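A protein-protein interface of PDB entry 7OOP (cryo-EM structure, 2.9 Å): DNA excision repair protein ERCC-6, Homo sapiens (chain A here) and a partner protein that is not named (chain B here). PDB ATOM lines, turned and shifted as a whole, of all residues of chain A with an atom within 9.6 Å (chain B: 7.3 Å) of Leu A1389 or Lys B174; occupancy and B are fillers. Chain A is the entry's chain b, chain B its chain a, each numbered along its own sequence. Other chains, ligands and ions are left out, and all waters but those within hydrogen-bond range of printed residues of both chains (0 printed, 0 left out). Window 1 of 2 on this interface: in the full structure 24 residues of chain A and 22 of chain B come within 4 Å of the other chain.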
ATOM      1  N   CYS A 732       3.521  40.207   5.292  1.00  0.00           N
ATOM      2  CA  CYS A 732       2.884  38.936   5.605  1.00  0.00           C
ATOM      3  C   CYS A 732       3.889  37.800   5.561  1.00  0.00           C
ATOM      4  O   CYS A 732       3.902  36.936   6.440  1.00  0.00           O
ATOM      5  CB  CYS A 732       1.740  38.672   4.634  1.00  0.00           C
ATOM      6  SG  CYS A 732       0.368  39.833   4.767  1.00  0.00           S
ATOM      7  N   VAL A 733       4.750  37.789   4.547  1.00  0.00           N
ATOM      8  CA  VAL A 733       5.732  36.714   4.442  1.00  0.00           C
ATOM      9  C   VAL A 733       6.657  36.718   5.648  1.00  0.00           C
ATOM     10  O   VAL A 733       6.921  35.673   6.242  1.00  0.00           O
ATOM     11  CB  VAL A 733       6.519  36.843   3.128  1.00  0.00           C
ATOM     12  CG1 VAL A 733       7.742  35.962   3.147  1.00  0.00           C
ATOM     13  CG2 VAL A 733       5.636  36.493   1.959  1.00  0.00           C
ATOM     14  N   ASP A 736       4.719  35.455   8.857  1.00  0.00           N
ATOM     15  CA  ASP A 736       4.557  34.010   8.959  1.00  0.00           C
ATOM     16  C   ASP A 736       5.894  33.286   9.013  1.00  0.00           C
ATOM     17  O   ASP A 736       5.962  32.170   9.527  1.00  0.00           O
ATOM     18  CB  ASP A 736       3.684  33.469   7.819  1.00  0.00           C
ATOM     19  CG  ASP A 736       2.326  34.167   7.718  1.00  0.00           C
ATOM     20  OD1 ASP A 736       2.218  35.277   7.166  1.00  0.00           O
ATOM     21  OD2 ASP A 736       1.338  33.571   8.192  1.00  0.00           O
ATOM     22  N   THR A 737       6.957  33.884   8.489  1.00  0.00           N
ATOM     23  CA  THR A 737       8.273  33.279   8.641  1.00  0.00           C
ATOM     24  C   THR A 737       8.729  33.305  10.090  1.00  0.00           C
ATOM     25  O   THR A 737       9.311  32.333  10.573  1.00  0.00           O
ATOM     26  CB  THR A 737       9.287  33.992   7.752  1.00  0.00           C
ATOM     27  OG1 THR A 737       8.888  33.869   6.386  1.00  0.00           O
ATOM     28  CG2 THR A 737      10.674  33.409   7.917  1.00  0.00           C
ATOM     29  N   ASN A 739       6.754  33.530  12.714  1.00  0.00           N
ATOM     30  CA  ASN A 739       5.674  33.183  13.634  1.00  0.00           C
ATOM     31  C   ASN A 739       6.055  32.118  14.648  1.00  0.00           C
ATOM     32  O   ASN A 739       5.812  32.328  15.845  1.00  0.00           O
ATOM     33  CB  ASN A 739       4.444  32.761  12.828  1.00  0.00           C
ATOM     34  CG  ASN A 739       3.208  32.600  13.685  1.00  0.00           C
ATOM     35  OD1 ASN A 739       3.074  33.232  14.733  1.00  0.00           O
ATOM     36  ND2 ASN A 739       2.291  31.752  13.239  1.00  0.00           N
ATOM     37  N   PRO A1383      -2.285  16.251   5.186  1.00  0.00           N
ATOM     38  CA  PRO A1383      -1.526  16.905   4.119  1.00  0.00           C
ATOM     39  C   PRO A1383      -2.383  17.886   3.337  1.00  0.00           C
ATOM     40  O   PRO A1383      -3.552  17.600   3.096  1.00  0.00           O
ATOM     41  CB  PRO A1383      -1.091  15.739   3.236  1.00  0.00           C
ATOM     42  CG  PRO A1383      -2.135  14.708   3.431  1.00  0.00           C
ATOM     43  CD  PRO A1383      -2.721  14.898   4.803  1.00  0.00           C
ATOM     44  N   LEU A1384      -1.818  19.024   2.951  1.00  0.00           N
ATOM     45  CA  LEU A1384      -2.572  19.989   2.168  1.00  0.00           C
ATOM     46  C   LEU A1384      -2.932  19.376   0.830  1.00  0.00           C
ATOM     47  O   LEU A1384      -2.080  18.789   0.160  1.00  0.00           O
ATOM     48  CB  LEU A1384      -1.759  21.261   1.960  1.00  0.00           C
ATOM     49  CG  LEU A1384      -1.680  22.227   3.141  1.00  0.00           C
ATOM     50  CD1 LEU A1384      -0.807  21.674   4.261  1.00  0.00           C
ATOM     51  CD2 LEU A1384      -1.162  23.572   2.675  1.00  0.00           C
ATOM     52  N   ALA A1385      -4.191  19.507   0.433  1.00  0.00           N
ATOM     53  CA  ALA A1385      -4.652  18.803  -0.759  1.00  0.00           C
ATOM     54  C   ALA A1385      -4.504  19.650  -2.014  1.00  0.00           C
ATOM     55  O   ALA A1385      -5.436  19.780  -2.804  1.00  0.00           O
ATOM     56  CB  ALA A1385      -6.097  18.359  -0.576  1.00  0.00           C
ATOM     57  N   SER A1386      -3.332  20.259  -2.191  1.00  0.00           N
ATOM     58  CA  SER A1386      -2.906  20.827  -3.465  1.00  0.00           C
ATOM     59  C   SER A1386      -3.913  21.776  -4.096  1.00  0.00           C
ATOM     60  O   SER A1386      -3.836  22.028  -5.296  1.00  0.00           O
ATOM     61  CB  SER A1386      -2.594  19.711  -4.462  1.00  0.00           C
ATOM     62  OG  SER A1386      -2.308  20.224  -5.754  1.00  0.00           O
ATOM     63  N   SER A1387      -4.880  22.257  -3.339  1.00  0.00           N
ATOM     64  CA  SER A1387      -5.769  23.312  -3.782  1.00  0.00           C
ATOM     65  C   SER A1387      -5.800  24.453  -2.795  1.00  0.00           C
ATOM     66  O   SER A1387      -5.772  25.613  -3.194  1.00  0.00           O
ATOM     67  CB  SER A1387      -7.184  22.767  -3.974  1.00  0.00           C
ATOM     68  OG  SER A1387      -7.217  21.819  -5.023  1.00  0.00           O
ATOM     69  N   SER A1388      -5.833  24.135  -1.506  1.00  0.00           N
ATOM     70  CA  SER A1388      -5.546  25.142  -0.500  1.00  0.00           C
ATOM     71  C   SER A1388      -4.135  25.670  -0.680  1.00  0.00           C
ATOM     72  O   SER A1388      -3.882  26.866  -0.513  1.00  0.00           O
ATOM     73  CB  SER A1388      -5.733  24.550   0.895  1.00  0.00           C
ATOM     74  OG  SER A1388      -4.919  23.406   1.061  1.00  0.00           O
ATOM     75  N   LEU A1389      -3.204  24.794  -1.037  1.00  0.00           N
ATOM     76  CA  LEU A1389      -1.849  25.246  -1.302  1.00  0.00           C
ATOM     77  C   LEU A1389      -1.834  26.175  -2.505  1.00  0.00           C
ATOM     78  O   LEU A1389      -1.333  27.301  -2.433  1.00  0.00           O
ATOM     79  CB  LEU A1389      -0.948  24.034  -1.520  1.00  0.00           C
ATOM     80  CG  LEU A1389       0.565  24.207  -1.606  1.00  0.00           C
ATOM     81  CD1 LEU A1389       1.116  24.727  -0.300  1.00  0.00           C
ATOM     82  CD2 LEU A1389       1.220  22.892  -1.982  1.00  0.00           C
ATOM     83  N   LEU A1390      -2.456  25.751  -3.597  1.00  0.00           N
ATOM     84  CA  LEU A1390      -2.527  26.600  -4.777  1.00  0.00           C
ATOM     85  C   LEU A1390      -3.362  27.845  -4.515  1.00  0.00           C
ATOM     86  O   LEU A1390      -3.048  28.924  -5.026  1.00  0.00           O
ATOM     87  CB  LEU A1390      -3.099  25.804  -5.942  1.00  0.00           C
ATOM     88  CG  LEU A1390      -2.133  24.915  -6.719  1.00  0.00           C
ATOM     89  CD1 LEU A1390      -2.937  24.060  -7.626  1.00  0.00           C
ATOM     90  CD2 LEU A1390      -1.164  25.715  -7.558  1.00  0.00           C
ATOM     91  N   ALA A1391      -4.431  27.719  -3.730  1.00  0.00           N
ATOM     92  CA  ALA A1391      -5.254  28.883  -3.442  1.00  0.00           C
ATOM     93  C   ALA A1391      -4.461  29.930  -2.679  1.00  0.00           C
ATOM     94  O   ALA A1391      -4.494  31.115  -3.020  1.00  0.00           O
ATOM     95  CB  ALA A1391      -6.488  28.470  -2.650  1.00  0.00           C
ATOM     96  N   LYS A1392      -3.717  29.505  -1.665  1.00  0.00           N
ATOM     97  CA  LYS A1392      -2.906  30.442  -0.910  1.00  0.00           C
ATOM     98  C   LYS A1392      -1.822  31.042  -1.781  1.00  0.00           C
ATOM     99  O   LYS A1392      -1.535  32.240  -1.684  1.00  0.00           O
ATOM    100  CB  LYS A1392      -2.293  29.743   0.294  1.00  0.00           C
ATOM    101  CG  LYS A1392      -3.305  29.464   1.370  1.00  0.00           C
ATOM    102  CD  LYS A1392      -2.720  28.679   2.521  1.00  0.00           C
ATOM    103  CE  LYS A1392      -3.803  28.391   3.540  1.00  0.00           C
ATOM    104  NZ  LYS A1392      -3.288  27.787   4.791  1.00  0.00           N
ATOM    105  N   MET A1393      -1.213  30.238  -2.653  1.00  0.00           N
ATOM    106  CA  MET A1393      -0.169  30.804  -3.494  1.00  0.00           C
ATOM    107  C   MET A1393      -0.738  31.865  -4.421  1.00  0.00           C
ATOM    108  O   MET A1393      -0.238  32.993  -4.455  1.00  0.00           O
ATOM    109  CB  MET A1393       0.577  29.720  -4.281  1.00  0.00           C
ATOM    110  CG  MET A1393       1.391  28.793  -3.393  1.00  0.00           C
ATOM    111  SD  MET A1393       2.368  27.550  -4.232  1.00  0.00           S
ATOM    112  CE  MET A1393       1.059  26.484  -4.716  1.00  0.00           C
ATOM    113  N   ARG A1394      -1.825  31.559  -5.127  1.00  0.00           N
ATOM    114  CA  ARG A1394      -2.359  32.540  -6.062  1.00  0.00           C
ATOM    115  C   ARG A1394      -2.887  33.765  -5.333  1.00  0.00           C
ATOM    116  O   ARG A1394      -2.780  34.886  -5.847  1.00  0.00           O
ATOM    117  CB  ARG A1394      -3.448  31.912  -6.929  1.00  0.00           C
ATOM    118  CG  ARG A1394      -4.697  31.495  -6.179  1.00  0.00           C
ATOM    119  CD  ARG A1394      -5.797  31.052  -7.123  1.00  0.00           C
ATOM    120  NE  ARG A1394      -5.401  29.897  -7.926  1.00  0.00           N
ATOM    121  CZ  ARG A1394      -4.914  29.946  -9.164  1.00  0.00           C
ATOM    122  NH1 ARG A1394      -4.734  31.101  -9.795  1.00  0.00           N
ATOM    123  NH2 ARG A1394      -4.595  28.819  -9.782  1.00  0.00           N
ATOM    124  N   ALA A1395      -3.431  33.581  -4.129  1.00  0.00           N
ATOM    125  CA  ALA A1395      -3.858  34.724  -3.335  1.00  0.00           C
ATOM    126  C   ALA A1395      -2.679  35.630  -3.024  1.00  0.00           C
ATOM    127  O   ALA A1395      -2.731  36.836  -3.271  1.00  0.00           O
ATOM    128  CB  ALA A1395      -4.525  34.246  -2.048  1.00  0.00           C
ATOM    129  N   ARG A1396      -1.590  35.060  -2.507  1.00  0.00           N
ATOM    130  CA  ARG A1396      -0.431  35.881  -2.186  1.00  0.00           C
ATOM    131  C   ARG A1396       0.151  36.539  -3.423  1.00  0.00           C
ATOM    132  O   ARG A1396       0.667  37.656  -3.341  1.00  0.00           O
ATOM    133  CB  ARG A1396       0.646  35.047  -1.508  1.00  0.00           C
ATOM    134  CG  ARG A1396       0.281  34.580  -0.128  1.00  0.00           C
ATOM    135  CD  ARG A1396       1.446  33.870   0.502  1.00  0.00           C
ATOM    136  NE  ARG A1396       1.724  32.600  -0.159  1.00  0.00           N
ATOM    137  CZ  ARG A1396       2.775  32.337  -0.928  1.00  0.00           C
ATOM    138  NH1 ARG A1396       3.696  33.250  -1.199  1.00  0.00           N
ATOM    139  NH2 ARG A1396       2.900  31.130  -1.436  1.00  0.00           N
ATOM    140  N   ASN A1397       0.086  35.871  -4.571  1.00  0.00           N
ATOM    141  CA  ASN A1397       0.719  36.425  -5.760  1.00  0.00           C
ATOM    142  C   ASN A1397      -0.107  37.517  -6.408  1.00  0.00           C
ATOM    143  O   ASN A1397       0.466  38.423  -7.022  1.00  0.00           O
ATOM    144  CB  ASN A1397       1.011  35.332  -6.775  1.00  0.00           C
ATOM    145  CG  ASN A1397       2.007  34.333  -6.261  1.00  0.00           C
ATOM    146  OD1 ASN A1397       1.689  33.171  -6.062  1.00  0.00           O
ATOM    147  ND2 ASN A1397       3.227  34.787  -6.025  1.00  0.00           N
ATOM    148  N   TYR B 108       4.097  17.345  -7.100  1.00  0.00           N
ATOM    149  CA  TYR B 108       3.792  17.536  -5.712  1.00  0.00           C
ATOM    150  C   TYR B 108       3.447  16.184  -5.126  1.00  0.00           C
ATOM    151  O   TYR B 108       2.559  15.506  -5.659  1.00  0.00           O
ATOM    152  CB  TYR B 108       2.624  18.466  -5.557  1.00  0.00           C
ATOM    153  CG  TYR B 108       2.230  18.717  -4.140  1.00  0.00           C
ATOM    154  CD1 TYR B 108       3.117  19.249  -3.241  1.00  0.00           C
ATOM    155  CD2 TYR B 108       0.956  18.436  -3.704  1.00  0.00           C
ATOM    156  CE1 TYR B 108       2.759  19.472  -1.953  1.00  0.00           C
ATOM    157  CE2 TYR B 108       0.588  18.666  -2.419  1.00  0.00           C
ATOM    158  CZ  TYR B 108       1.493  19.183  -1.546  1.00  0.00           C
ATOM    159  OH  TYR B 108       1.118  19.411  -0.248  1.00  0.00           O
ATOM    160  N   PRO B 109       4.094  15.738  -4.064  1.00  0.00           N
ATOM    161  CA  PRO B 109       3.620  14.526  -3.416  1.00  0.00           C
ATOM    162  C   PRO B 109       2.262  14.769  -2.784  1.00  0.00           C
ATOM    163  O   PRO B 109       1.881  15.888  -2.452  1.00  0.00           O
ATOM    164  CB  PRO B 109       4.682  14.248  -2.366  1.00  0.00           C
ATOM    165  CG  PRO B 109       5.267  15.548  -2.102  1.00  0.00           C
ATOM    166  CD  PRO B 109       5.233  16.315  -3.345  1.00  0.00           C
ATOM    167  N   MET B 114      -0.485  19.658  -8.673  1.00  0.00           N
ATOM    168  CA  MET B 114       0.545  20.676  -8.624  1.00  0.00           C
ATOM    169  C   MET B 114       1.869  20.026  -8.958  1.00  0.00           C
ATOM    170  O   MET B 114       2.094  18.870  -8.610  1.00  0.00           O
ATOM    171  CB  MET B 114       0.596  21.289  -7.233  1.00  0.00           C
ATOM    172  CG  MET B 114       1.104  22.680  -7.158  1.00  0.00           C
ATOM    173  SD  MET B 114       1.866  22.989  -5.569  1.00  0.00           S
ATOM    174  CE  MET B 114       3.450  22.222  -5.778  1.00  0.00           C
ATOM    175  N   VAL B 126       6.296  27.017  -9.510  1.00  0.00           N
ATOM    176  CA  VAL B 126       5.265  26.081  -9.098  1.00  0.00           C
ATOM    177  C   VAL B 126       4.120  26.198 -10.077  1.00  0.00           C
ATOM    178  O   VAL B 126       3.608  27.292 -10.315  1.00  0.00           O
ATOM    179  CB  VAL B 126       4.781  26.351  -7.671  1.00  0.00           C
ATOM    180  CG1 VAL B 126       3.775  25.305  -7.284  1.00  0.00           C
ATOM    181  CG2 VAL B 126       5.944  26.363  -6.708  1.00  0.00           C
ATOM    182  N   ALA B 135       1.678  29.092 -10.378  1.00  0.00           N
ATOM    183  CA  ALA B 135       1.026  29.628  -9.199  1.00  0.00           C
ATOM    184  C   ALA B 135       1.983  30.349  -8.274  1.00  0.00           C
ATOM    185  O   ALA B 135       1.531  31.058  -7.379  1.00  0.00           O
ATOM    186  CB  ALA B 135       0.324  28.520  -8.417  1.00  0.00           C
ATOM    187  N   ASP B 136       3.280  30.137  -8.426  1.00  0.00           N
ATOM    188  CA  ASP B 136       4.266  30.844  -7.634  1.00  0.00           C
ATOM    189  C   ASP B 136       5.588  30.752  -8.364  1.00  0.00           C
ATOM    190  O   ASP B 136       5.807  29.843  -9.160  1.00  0.00           O
ATOM    191  CB  ASP B 136       4.381  30.261  -6.226  1.00  0.00           C
ATOM    192  CG  ASP B 136       5.102  31.178  -5.282  1.00  0.00           C
ATOM    193  OD1 ASP B 136       5.627  32.209  -5.745  1.00  0.00           O
ATOM    194  OD2 ASP B 136       5.156  30.866  -4.075  1.00  0.00           O
ATOM    195  N   PHE B 138       9.833  31.354  -7.377  1.00  0.00           N
ATOM    196  CA  PHE B 138      10.896  31.663  -6.442  1.00  0.00           C
ATOM    197  C   PHE B 138      12.132  31.982  -7.256  1.00  0.00           C
ATOM    198  O   PHE B 138      12.695  31.103  -7.912  1.00  0.00           O
ATOM    199  CB  PHE B 138      11.144  30.502  -5.495  1.00  0.00           C
ATOM    200  CG  PHE B 138      10.024  30.253  -4.563  1.00  0.00           C
ATOM    201  CD1 PHE B 138       8.934  29.518  -4.955  1.00  0.00           C
ATOM    202  CD2 PHE B 138      10.060  30.752  -3.293  1.00  0.00           C
ATOM    203  CE1 PHE B 138       7.908  29.291  -4.098  1.00  0.00           C
ATOM    204  CE2 PHE B 138       9.031  30.524  -2.426  1.00  0.00           C
ATOM    205  CZ  PHE B 138       7.954  29.795  -2.828  1.00  0.00           C
ATOM    206  N   MET B 149      11.056  18.181  -3.121  1.00  0.00           N
ATOM    207  CA  MET B 149      10.058  18.217  -2.065  1.00  0.00           C
ATOM    208  C   MET B 149      10.080  16.909  -1.303  1.00  0.00           C
ATOM    209  O   MET B 149      10.305  15.849  -1.886  1.00  0.00           O
ATOM    210  CB  MET B 149       8.661  18.423  -2.626  1.00  0.00           C
ATOM    211  CG  MET B 149       8.332  19.829  -2.919  1.00  0.00           C
ATOM    212  SD  MET B 149       6.691  20.072  -3.583  1.00  0.00           S
ATOM    213  CE  MET B 149       6.958  19.459  -5.230  1.00  0.00           C
ATOM    214  N   LYS B 155       3.477  17.439   7.152  1.00  0.00           N
ATOM    215  CA  LYS B 155       3.430  18.627   7.995  1.00  0.00           C
ATOM    216  C   LYS B 155       3.961  19.863   7.281  1.00  0.00           C
ATOM    217  O   LYS B 155       3.237  20.850   7.124  1.00  0.00           O
ATOM    218  CB  LYS B 155       4.229  18.371   9.276  1.00  0.00           C
ATOM    219  CG  LYS B 155       3.708  17.202  10.089  1.00  0.00           C
ATOM    220  CD  LYS B 155       2.934  17.673  11.311  1.00  0.00           C
ATOM    221  CE  LYS B 155       2.296  16.503  12.037  1.00  0.00           C
ATOM    222  NZ  LYS B 155       1.074  16.021  11.335  1.00  0.00           N
ATOM    223  N   HIS B 156       5.214  19.824   6.843  1.00  0.00           N
ATOM    224  CA  HIS B 156       5.841  20.940   6.154  1.00  0.00           C
ATOM    225  C   HIS B 156       5.885  20.641   4.669  1.00  0.00           C
ATOM    226  O   HIS B 156       5.895  19.483   4.252  1.00  0.00           O
ATOM    227  CB  HIS B 156       7.255  21.183   6.661  1.00  0.00           C
ATOM    228  CG  HIS B 156       8.183  20.043   6.410  1.00  0.00           C
ATOM    229  ND1 HIS B 156       8.891  19.895   5.237  1.00  0.00           N
ATOM    230  CD2 HIS B 156       8.457  18.950   7.153  1.00  0.00           C
ATOM    231  CE1 HIS B 156       9.611  18.790   5.299  1.00  0.00           C
ATOM    232  NE2 HIS B 156       9.364  18.199   6.452  1.00  0.00           N
ATOM    233  N   CYS B 157       5.909  21.698   3.875  1.00  0.00           N
ATOM    234  CA  CYS B 157       5.959  21.603   2.427  1.00  0.00           C
ATOM    235  C   CYS B 157       7.105  22.441   1.901  1.00  0.00           C
ATOM    236  O   CYS B 157       6.954  23.264   1.004  1.00  0.00           O
ATOM    237  CB  CYS B 157       4.634  22.020   1.823  1.00  0.00           C
ATOM    238  SG  CYS B 157       4.538  21.794   0.048  1.00  0.00           S
ATOM    239  N   LEU B 158       8.278  22.250   2.486  1.00  0.00           N
ATOM    240  CA  LEU B 158       9.470  22.948   2.042  1.00  0.00           C
ATOM    241  C   LEU B 158      10.021  22.326   0.775  1.00  0.00           C
ATOM    242  O   LEU B 158       9.886  21.124   0.551  1.00  0.00           O
ATOM    243  CB  LEU B 158      10.550  22.907   3.115  1.00  0.00           C
ATOM    244  CG  LEU B 158      10.125  23.226   4.530  1.00  0.00           C
ATOM    245  CD1 LEU B 158      11.206  22.813   5.474  1.00  0.00           C
ATOM    246  CD2 LEU B 158       9.854  24.691   4.638  1.00  0.00           C
ATOM    247  N   CYS B 171      12.523  26.628   0.463  1.00  0.00           N
ATOM    248  CA  CYS B 171      11.400  27.453   0.033  1.00  0.00           C
ATOM    249  C   CYS B 171      10.101  26.806   0.473  1.00  0.00           C
ATOM    250  O   CYS B 171       9.751  25.727  -0.007  1.00  0.00           O
ATOM    251  CB  CYS B 171      11.405  27.636  -1.474  1.00  0.00           C
ATOM    252  SG  CYS B 171      12.995  28.071  -2.102  1.00  0.00           S
ATOM    253  N   ASP B 172       9.369  27.497   1.338  1.00  0.00           N
ATOM    254  CA  ASP B 172       8.137  26.989   1.922  1.00  0.00           C
ATOM    255  C   ASP B 172       6.996  27.319   0.972  1.00  0.00           C
ATOM    256  O   ASP B 172       6.697  28.487   0.745  1.00  0.00           O
ATOM    257  CB  ASP B 172       7.932  27.619   3.297  1.00  0.00           C
ATOM    258  CG  ASP B 172       6.797  27.004   4.062  1.00  0.00           C
ATOM    259  OD1 ASP B 172       6.134  26.101   3.521  1.00  0.00           O
ATOM    260  OD2 ASP B 172       6.556  27.439   5.205  1.00  0.00           O
ATOM    261  N   LEU B 173       6.374  26.298   0.390  1.00  0.00           N
ATOM    262  CA  LEU B 173       5.273  26.565  -0.529  1.00  0.00           C
ATOM    263  C   LEU B 173       4.045  27.034   0.226  1.00  0.00           C
ATOM    264  O   LEU B 173       3.340  27.940  -0.227  1.00  0.00           O
ATOM    265  CB  LEU B 173       4.962  25.326  -1.355  1.00  0.00           C
ATOM    266  CG  LEU B 173       6.054  24.826  -2.294  1.00  0.00           C
ATOM    267  CD1 LEU B 173       5.451  23.858  -3.277  1.00  0.00           C
ATOM    268  CD2 LEU B 173       6.777  25.930  -3.039  1.00  0.00           C
ATOM    269  N   LYS B 174       3.760  26.426   1.372  1.00  0.00           N
ATOM    270  CA  LYS B 174       2.944  27.101   2.364  1.00  0.00           C
ATOM    271  C   LYS B 174       3.579  28.453   2.632  1.00  0.00           C
ATOM    272  O   LYS B 174       4.799  28.584   2.542  1.00  0.00           O
ATOM    273  CB  LYS B 174       2.875  26.279   3.646  1.00  0.00           C
ATOM    274  CG  LYS B 174       1.989  26.855   4.719  1.00  0.00           C
ATOM    275  CD  LYS B 174       0.527  26.760   4.343  1.00  0.00           C
ATOM    276  CE  LYS B 174      -0.343  27.287   5.460  1.00  0.00           C
ATOM    277  NZ  LYS B 174      -0.371  26.354   6.613  1.00  0.00           N
ATOM    278  N   SER B 175       2.768  29.421   3.064  1.00  0.00           N
ATOM    279  CA  SER B 175       2.962  30.838   2.754  1.00  0.00           C
ATOM    280  C   SER B 175       4.433  31.216   2.605  1.00  0.00           C
ATOM    281  O   SER B 175       5.247  30.964   3.495  1.00  0.00           O
ATOM    282  CB  SER B 175       2.288  31.686   3.837  1.00  0.00           C
ATOM    283  OG  SER B 175       2.315  33.065   3.520  1.00  0.00           O
ATOM    284  N   GLY B 176       4.756  31.837   1.475  1.00  0.00           N
ATOM    285  CA  GLY B 176       6.047  31.720   0.824  1.00  0.00           C
ATOM    286  C   GLY B 176       7.240  32.352   1.498  1.00  0.00           C
ATOM    287  O   GLY B 176       7.362  33.577   1.507  1.00  0.00           O
ATOM    288  N   SER B 177       8.152  31.538   2.018  1.00  0.00           N
ATOM    289  CA  SER B 177       9.335  32.024   2.721  1.00  0.00           C
ATOM    290  C   SER B 177      10.554  31.324   2.141  1.00  0.00           C
ATOM    291  O   SER B 177      10.816  30.164   2.459  1.00  0.00           O
ATOM    292  CB  SER B 177       9.222  31.781   4.222  1.00  0.00           C
ATOM    293  OG  SER B 177       9.188  30.403   4.527  1.00  0.00           O
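The backbone carbonyl oxygen of Ala B135 lies close to the side-chain amide oxygen of Asn A1397 (2.5 Å).
O of Leu A1384 lies within hydrogen-bond range of OH of Tyr B108 (3.3 Å).
The backbone carbonyl oxygen (O) of Leu B173 is in hydrogen-bond range of the guanidinium group (NH2) of Arg A1396 (3.4 Å).
The guanidinium group (NH2) of Arg A1396 is in salt-bridge range of the side-chain carboxylate (OD2) of Asp B136 (3.5 Å).
The backbone NH (N) of Gly B176 lies close to the guanidinium group (NH1) of Arg A1396 (3.2 Å).
N of Met B114 lies close to OG of Ser A1386, 3.5 Å away.
Of the 19 printed residues of chain B, 10 touch a printed residue of chain A.
Printed residues of chain B that touch a printed residue of chain A: Tyr B108, Met B114, Val B126, Ala B135, Asp B136, Leu B173, Lys B174, Ser B175, Gly B176 and Ser B177.
Hydrophobic or aromatic side chains of chain B within 4 Å of the printed part of chain A: Tyr B108, Met B114, Val B126 and Ala B135.
Of the 20 printed residues of chain A, 10 touch a printed residue of chain B.
Among the printed residues, Asp or Glu carboxylates within 4 Å of a Lys or Arg side-chain nitrogen of the other chain: Arg A1396 with Asp B136 (3.5 Å).
Of chain B, only Tyr B108, Met B114, Leu B173 and Lys B174 come within 4 Å of Leu A1389.
Of chain A, only Leu A1384, Leu A1389 and Lys A1392 come within 4 Å of Lys B174.
No residue of chain B comes within 4 Å of Ser A1388.
Cys B157 touches none of the printed residues of chain A.
No residue of chain A comes within 4 Å of Asp B172.
Printed residues of chain A within 4 Å of Leu B173: Leu A1389 (3.8 Å), Met A1393 (3.8 Å) and Arg A1396 (3.4 Å).
Of chain A, only Arg A1396 comes within 4 Å of Ser B175.
Of the printed residues of chain B, Lys A1392 touches Lys B174 (3.1 Å).
Of the printed residues of chain A, Met B114 touches Ser A1386, Leu A1389, Leu A1390 and Met A1393.
Of the printed residues of chain B, Leu A1390 touches Met B114 and Ala B135.
Of the printed residues of chain B, Thr A737 touches Ser B177 (3.0 Å).
Lys B155 touches none of the printed residues of chain A.
The nearest residue of chain A that does not touch Lys B174 is Arg A1396 (4.9 Å).
Val A733 touches Gly B176 (CG1 to O, 2.9 Å).
Ser A1386 touches Tyr B108.
Leu A1389 touches Met B114 (CD2 to SD, 3.6 Å).
CD1 of Leu A1389 touches N of Lys B174 (3.6 Å).
CD2 of Leu A1390 touches CB of Ala B135, at 3.3 Å.
Lys B174 touches Lys A1392.
SD of Met B114 touches CE of Met A1393 (3.7 Å).
Met A1393 touches Val B126.
Met A1393 touches Ala B135 (CB to O, 3.5 Å).
Asp B136 touches Asn A1397.
The backbone carbonyl oxygen (O) of Ser B177 sits at hydrogen-bond distance from the backbone NH (N) of Asp B172 (3.2 Å).
The side-chain carboxylate (OD1) of Asp B172 sits at hydrogen-bond distance from the backbone NH (N) of Lys B174.
N of Val B126 is in hydrogen-bond range of O of Asp B136 (2.9 Å).
The backbone carbonyl oxygen (O) of Met A1393 lies close to the side-chain amide oxygen (OD1) of Asn A1397.
O of Val A733 lies within hydrogen-bond range of OG1 of Thr A737 (2.7 Å).
The backbone carbonyl oxygen (O) of Val B126 is in hydrogen-bond range of the backbone NH (N) of Ala B135 (2.6 Å).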
